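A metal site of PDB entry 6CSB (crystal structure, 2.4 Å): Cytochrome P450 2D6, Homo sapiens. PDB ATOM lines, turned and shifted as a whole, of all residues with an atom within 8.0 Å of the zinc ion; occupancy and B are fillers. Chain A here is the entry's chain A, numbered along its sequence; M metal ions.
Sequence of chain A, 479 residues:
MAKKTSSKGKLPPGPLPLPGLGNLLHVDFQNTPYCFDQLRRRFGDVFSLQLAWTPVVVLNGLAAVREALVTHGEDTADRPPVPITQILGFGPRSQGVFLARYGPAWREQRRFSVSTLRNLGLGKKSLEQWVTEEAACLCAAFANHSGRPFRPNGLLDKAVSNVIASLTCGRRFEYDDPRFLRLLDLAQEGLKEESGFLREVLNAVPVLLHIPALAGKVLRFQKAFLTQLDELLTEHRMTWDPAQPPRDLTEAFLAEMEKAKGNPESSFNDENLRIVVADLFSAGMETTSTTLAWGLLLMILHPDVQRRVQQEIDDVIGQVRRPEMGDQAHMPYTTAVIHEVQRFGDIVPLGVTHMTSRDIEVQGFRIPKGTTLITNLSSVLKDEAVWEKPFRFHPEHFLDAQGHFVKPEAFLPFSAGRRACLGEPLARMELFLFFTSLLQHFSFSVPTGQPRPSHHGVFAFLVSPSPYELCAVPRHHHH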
ATOM      1  N   ALA A 165       0.349 -15.598  14.738  1.00  0.00           N
ATOM      2  CA  ALA A 165       0.583 -16.953  15.268  1.00  0.00           C
ATOM      3  C   ALA A 165       1.944 -17.040  15.932  1.00  0.00           C
ATOM      4  O   ALA A 165       2.079 -17.653  17.014  1.00  0.00           O
ATOM      5  CB  ALA A 165       0.466 -18.001  14.150  1.00  0.00           C
ATOM      6  N   SER A 166       2.956 -16.421  15.339  1.00  0.00           N
ATOM      7  CA  SER A 166       4.290 -16.429  15.930  1.00  0.00           C
ATOM      8  C   SER A 166       4.286 -15.690  17.262  1.00  0.00           C
ATOM      9  O   SER A 166       4.829 -16.189  18.254  1.00  0.00           O
ATOM     10  CB  SER A 166       5.319 -15.796  14.992  1.00  0.00           C
ATOM     11  OG  SER A 166       5.365 -16.496  13.775  1.00  0.00           O
ATOM     12  N   LEU A 167       3.731 -14.476  17.278  1.00  0.00           N
ATOM     13  CA  LEU A 167       3.633 -13.690  18.497  1.00  0.00           C
ATOM     14  C   LEU A 167       2.918 -14.462  19.595  1.00  0.00           C
ATOM     15  O   LEU A 167       3.371 -14.502  20.747  1.00  0.00           O
ATOM     16  CB  LEU A 167       2.884 -12.371  18.199  1.00  0.00           C
ATOM     17  CG  LEU A 167       2.219 -11.674  19.415  1.00  0.00           C
ATOM     18  CD1 LEU A 167       3.259 -11.141  20.383  1.00  0.00           C
ATOM     19  CD2 LEU A 167       1.264 -10.559  19.015  1.00  0.00           C
ATOM     20  N   THR A 168       1.791 -15.074  19.253  1.00  0.00           N
ATOM     21  CA  THR A 168       0.921 -15.618  20.269  1.00  0.00           C
ATOM     22  C   THR A 168       1.188 -17.086  20.560  1.00  0.00           C
ATOM     23  O   THR A 168       1.034 -17.493  21.709  1.00  0.00           O
ATOM     24  CB  THR A 168      -0.541 -15.427  19.865  1.00  0.00           C
ATOM     25  OG1 THR A 168      -0.802 -16.205  18.697  1.00  0.00           O
ATOM     26  CG2 THR A 168      -0.842 -13.948  19.584  1.00  0.00           C
ATOM     27  N   CYS A 169       1.590 -17.894  19.583  1.00  0.00           N
ATOM     28  CA  CYS A 169       1.815 -19.318  19.833  1.00  0.00           C
ATOM     29  C   CYS A 169       3.207 -19.812  19.485  1.00  0.00           C
ATOM     30  O   CYS A 169       3.468 -21.008  19.640  1.00  0.00           O
ATOM     31  CB  CYS A 169       0.795 -20.170  19.066  1.00  0.00           C
ATOM     32  SG  CYS A 169      -0.899 -19.959  19.618  1.00  0.00           S
ATOM     33  N   GLY A 170       4.104 -18.955  18.996  1.00  0.00           N
ATOM     34  CA  GLY A 170       5.454 -19.396  18.714  1.00  0.00           C
ATOM     35  C   GLY A 170       5.623 -20.336  17.540  1.00  0.00           C
ATOM     36  O   GLY A 170       6.623 -21.047  17.464  1.00  0.00           O
ATOM     37  N   ARG A 171       4.688 -20.343  16.596  1.00  0.00           N
ATOM     38  CA  ARG A 171       4.807 -21.151  15.391  1.00  0.00           C
ATOM     39  C   ARG A 171       4.285 -20.356  14.203  1.00  0.00           C
ATOM     40  O   ARG A 171       3.671 -19.287  14.368  1.00  0.00           O
ATOM     41  CB  ARG A 171       4.009 -22.469  15.532  1.00  0.00           C
ATOM     42  CG  ARG A 171       2.511 -22.272  15.637  1.00  0.00           C
ATOM     43  CD  ARG A 171       1.753 -23.555  15.331  1.00  0.00           C
ATOM     44  NE  ARG A 171       2.129 -24.071  14.020  1.00  0.00           N
ATOM     45  CZ  ARG A 171       1.775 -25.258  13.539  1.00  0.00           C
ATOM     46  NH1 ARG A 171       1.018 -26.099  14.262  1.00  0.00           N
ATOM     47  NH2 ARG A 171       2.190 -25.608  12.328  1.00  0.00           N
ATOM     48  N   HIS A 236      -0.637 -26.018  22.056  1.00  0.00           N
ATOM     49  CA  HIS A 236       0.471 -25.229  22.575  1.00  0.00           C
ATOM     50  C   HIS A 236       0.680 -25.522  24.059  1.00  0.00           C
ATOM     51  O   HIS A 236       1.816 -25.580  24.538  1.00  0.00           O
ATOM     52  CB  HIS A 236       0.222 -23.731  22.345  1.00  0.00           C
ATOM     53  CG  HIS A 236       1.433 -22.874  22.586  1.00  0.00           C
ATOM     54  ND1 HIS A 236       1.378 -21.502  22.706  1.00  0.00           N
ATOM     55  CD2 HIS A 236       2.745 -23.192  22.706  1.00  0.00           C
ATOM     56  CE1 HIS A 236       2.583 -21.016  22.877  1.00  0.00           C
ATOM     57  NE2 HIS A 236       3.437 -22.011  22.882  1.00  0.00           N
ATOM     58  N   ARG A 237      -0.414 -25.739  24.787  1.00  0.00           N
ATOM     59  CA  ARG A 237      -0.296 -26.104  26.191  1.00  0.00           C
ATOM     60  C   ARG A 237       0.567 -27.339  26.359  1.00  0.00           C
ATOM     61  O   ARG A 237       1.363 -27.427  27.294  1.00  0.00           O
ATOM     62  CB  ARG A 237      -1.681 -26.338  26.765  1.00  0.00           C
ATOM     63  CG  ARG A 237      -1.945 -25.654  28.077  1.00  0.00           C
ATOM     64  CD  ARG A 237      -3.432 -25.585  28.345  1.00  0.00           C
ATOM     65  NE  ARG A 237      -3.711 -24.834  29.555  1.00  0.00           N
ATOM     66  CZ  ARG A 237      -4.599 -23.843  29.617  1.00  0.00           C
ATOM     67  NH1 ARG A 237      -5.298 -23.506  28.537  1.00  0.00           N
ATOM     68  NH2 ARG A 237      -4.780 -23.208  30.767  1.00  0.00           N
ATOM     69  N   THR A 239       3.068 -28.433  24.423  1.00  0.00           N
ATOM     70  CA  THR A 239       4.488 -28.279  24.085  1.00  0.00           C
ATOM     71  C   THR A 239       5.192 -27.207  24.914  1.00  0.00           C
ATOM     72  O   THR A 239       6.422 -27.072  24.796  1.00  0.00           O
ATOM     73  CB  THR A 239       4.674 -27.950  22.617  1.00  0.00           C
ATOM     74  OG1 THR A 239       3.956 -26.748  22.315  1.00  0.00           O
ATOM     75  CG2 THR A 239       4.149 -29.086  21.752  1.00  0.00           C
ATOM     76  N   TRP A 240       4.461 -26.460  25.729  1.00  0.00           N
ATOM     77  CA  TRP A 240       5.059 -25.405  26.519  1.00  0.00           C
ATOM     78  C   TRP A 240       6.047 -25.978  27.534  1.00  0.00           C
ATOM     79  O   TRP A 240       5.751 -26.955  28.231  1.00  0.00           O
ATOM     80  CB  TRP A 240       3.969 -24.615  27.233  1.00  0.00           C
ATOM     81  CG  TRP A 240       4.448 -23.635  28.232  1.00  0.00           C
ATOM     82  CD1 TRP A 240       5.556 -22.836  28.160  1.00  0.00           C
ATOM     83  CD2 TRP A 240       3.829 -23.357  29.482  1.00  0.00           C
ATOM     84  NE1 TRP A 240       5.658 -22.071  29.302  1.00  0.00           N
ATOM     85  CE2 TRP A 240       4.601 -22.363  30.116  1.00  0.00           C
ATOM     86  CE3 TRP A 240       2.677 -23.837  30.117  1.00  0.00           C
ATOM     87  CZ2 TRP A 240       4.260 -21.843  31.374  1.00  0.00           C
ATOM     88  CZ3 TRP A 240       2.354 -23.333  31.382  1.00  0.00           C
ATOM     89  CH2 TRP A 240       3.138 -22.328  31.978  1.00  0.00           C
ATOM     90  N   ASP A 241       7.227 -25.368  27.600  1.00  0.00           N
ATOM     91  CA  ASP A 241       8.265 -25.775  28.543  1.00  0.00           C
ATOM     92  C   ASP A 241       8.368 -24.702  29.618  1.00  0.00           C
ATOM     93  O   ASP A 241       9.124 -23.731  29.443  1.00  0.00           O
ATOM     94  CB  ASP A 241       9.602 -25.966  27.828  1.00  0.00           C
ATOM     95  CG  ASP A 241      10.662 -26.508  28.740  1.00  0.00           C
ATOM     96  OD1 ASP A 241      10.369 -26.685  29.940  1.00  0.00           O
ATOM     97  OD2 ASP A 241      11.788 -26.777  28.257  1.00  0.00           O
ATOM     98  N   PRO A 245      12.314 -19.591  29.789  1.00  0.00           N
ATOM     99  CA  PRO A 245      11.608 -18.328  29.675  1.00  0.00           C
ATOM    100  C   PRO A 245      10.563 -18.408  28.576  1.00  0.00           C
ATOM    101  O   PRO A 245      10.749 -19.128  27.573  1.00  0.00           O
ATOM    102  CB  PRO A 245      12.728 -17.336  29.306  1.00  0.00           C
ATOM    103  CG  PRO A 245      13.979 -17.991  29.786  1.00  0.00           C
ATOM    104  CD  PRO A 245      13.757 -19.442  29.535  1.00  0.00           C
ATOM    105  N   PRO A 246       9.441 -17.716  28.743  1.00  0.00           N
ATOM    106  CA  PRO A 246       8.370 -17.810  27.739  1.00  0.00           C
ATOM    107  C   PRO A 246       8.884 -17.377  26.374  1.00  0.00           C
ATOM    108  O   PRO A 246       9.607 -16.387  26.244  1.00  0.00           O
ATOM    109  CB  PRO A 246       7.291 -16.870  28.272  1.00  0.00           C
ATOM    110  CG  PRO A 246       7.674 -16.561  29.689  1.00  0.00           C
ATOM    111  CD  PRO A 246       9.159 -16.669  29.737  1.00  0.00           C
ATOM    112  N   ARG A 247       8.538 -18.137  25.356  1.00  0.00           N
ATOM    113  CA  ARG A 247       9.041 -17.775  24.046  1.00  0.00           C
ATOM    114  C   ARG A 247       7.993 -17.062  23.207  1.00  0.00           C
ATOM    115  O   ARG A 247       8.284 -16.673  22.081  1.00  0.00           O
ATOM    116  CB  ARG A 247       9.594 -19.011  23.326  1.00  0.00           C
ATOM    117  CG  ARG A 247       8.639 -20.174  23.155  1.00  0.00           C
ATOM    118  CD  ARG A 247       9.328 -21.281  22.350  1.00  0.00           C
ATOM    119  NE  ARG A 247      10.038 -20.729  21.186  1.00  0.00           N
ATOM    120  CZ  ARG A 247       9.521 -20.623  19.966  1.00  0.00           C
ATOM    121  NH1 ARG A 247       8.293 -21.044  19.708  1.00  0.00           N
ATOM    122  NH2 ARG A 247      10.250 -20.091  18.986  1.00  0.00           N
ATOM    123  N   ASP A 248       6.796 -16.846  23.744  1.00  0.00           N
ATOM    124  CA  ASP A 248       5.733 -16.174  23.016  1.00  0.00           C
ATOM    125  C   ASP A 248       4.675 -15.705  24.022  1.00  0.00           C
ATOM    126  O   ASP A 248       4.768 -15.947  25.222  1.00  0.00           O
ATOM    127  CB  ASP A 248       5.165 -17.104  21.959  1.00  0.00           C
ATOM    128  CG  ASP A 248       4.754 -18.455  22.547  1.00  0.00           C
ATOM    129  OD1 ASP A 248       3.959 -18.470  23.518  1.00  0.00           O
ATOM    130  OD2 ASP A 248       5.256 -19.495  22.064  1.00  0.00           O
ATOM    131  N   LEU A 249       3.637 -15.057  23.514  1.00  0.00           N
ATOM    132  CA  LEU A 249       2.783 -14.321  24.427  1.00  0.00           C
ATOM    133  C   LEU A 249       1.939 -15.281  25.236  1.00  0.00           C
ATOM    134  O   LEU A 249       1.730 -15.060  26.441  1.00  0.00           O
ATOM    135  CB  LEU A 249       1.915 -13.318  23.640  1.00  0.00           C
ATOM    136  CG  LEU A 249       0.889 -12.496  24.438  1.00  0.00           C
ATOM    137  CD1 LEU A 249       0.803 -11.051  23.895  1.00  0.00           C
ATOM    138  CD2 LEU A 249      -0.462 -13.188  24.400  1.00  0.00           C
ATOM    139  N   THR A 250       1.482 -16.343  24.617  1.00  0.00           N
ATOM    140  CA  THR A 250       0.644 -17.287  25.339  1.00  0.00           C
ATOM    141  C   THR A 250       1.406 -17.968  26.468  1.00  0.00           C
ATOM    142  O   THR A 250       0.853 -18.241  27.529  1.00  0.00           O
ATOM    143  CB  THR A 250       0.083 -18.303  24.357  1.00  0.00           C
ATOM    144  OG1 THR A 250      -1.038 -17.710  23.711  1.00  0.00           O
ATOM    145  CG2 THR A 250      -0.317 -19.588  25.055  1.00  0.00           C
ATOM    146  N   GLU A 251       2.689 -18.221  26.267  1.00  0.00           N
ATOM    147  CA  GLU A 251       3.481 -18.787  27.358  1.00  0.00           C
ATOM    148  C   GLU A 251       3.607 -17.788  28.498  1.00  0.00           C
ATOM    149  O   GLU A 251       3.346 -18.127  29.669  1.00  0.00           O
ATOM    150  CB  GLU A 251       4.862 -19.222  26.829  1.00  0.00           C
ATOM    151  CG  GLU A 251       4.778 -20.472  25.926  1.00  0.00           C
ATOM    152  CD  GLU A 251       6.129 -20.984  25.441  1.00  0.00           C
ATOM    153  OE1 GLU A 251       7.163 -20.596  26.033  1.00  0.00           O
ATOM    154  OE2 GLU A 251       6.152 -21.746  24.471  1.00  0.00           O
ATOM    155  N   ALA A 252       3.985 -16.548  28.190  1.00  0.00           N
ATOM    156  CA  ALA A 252       4.024 -15.492  29.209  1.00  0.00           C
ATOM    157  C   ALA A 252       2.715 -15.455  29.973  1.00  0.00           C
ATOM    158  O   ALA A 252       2.697 -15.398  31.217  1.00  0.00           O
ATOM    159  CB  ALA A 252       4.317 -14.140  28.533  1.00  0.00           C
ATOM    160  N   LEU A 254       0.426 -17.901  30.287  1.00  0.00           N
ATOM    161  CA  LEU A 254       0.247 -19.113  31.078  1.00  0.00           C
ATOM    162  C   LEU A 254       1.078 -19.060  32.358  1.00  0.00           C
ATOM    163  O   LEU A 254       0.621 -19.486  33.425  1.00  0.00           O
ATOM    164  CB  LEU A 254       0.610 -20.337  30.242  1.00  0.00           C
ATOM    165  CG  LEU A 254      -0.413 -20.738  29.173  1.00  0.00           C
ATOM    166  CD1 LEU A 254       0.234 -21.700  28.180  1.00  0.00           C
ATOM    167  CD2 LEU A 254      -1.681 -21.358  29.764  1.00  0.00           C
HETATM  168 ZN    ZN M   1       5.152 -21.440  22.754  1.00  0.00          ZN
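The backbone carbonyl oxygen of Cys 169 lies close to a ring nitrogen (NE2) of His 236, 3.4 Å away.
OG1 of Thr 239 is in hydrogen-bond range of O of His 236, 3.3 Å away.
The side-chain carboxylate (OE1) of Glu 251 lies within hydrogen-bond range of the backbone NH (N) of Arg 247 (2.9 Å).
The backbone NH (N) of Gly 170 lies close to the side-chain carboxylate (OD2) of Asp 248.
The backbone NH (N) of Thr 250 lies close to the side-chain carboxylate (OD1) of Asp 248.
NH1 of Arg 247 sits at hydrogen-bond distance from O of Gly 170 (2.8 Å).
Residues that only touch the zinc ion: Cys 169 (3.6 Å) and Arg 247 (3.7 Å).
Five residues have an atom within 4 Å of the zinc ion: Cys 169, His 236, Arg 247, Asp 248 and Glu 251.
The nearest printed residue that does not touch the zinc ion is Gly 170 (4.5 Å).
NE2 of His 236 binds the zinc ion (1.8 Å).
The zinc ion is bound by OE2 of Glu 251.
The zinc ion is bound by OD2 of Asp 248 (2.1 Å).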
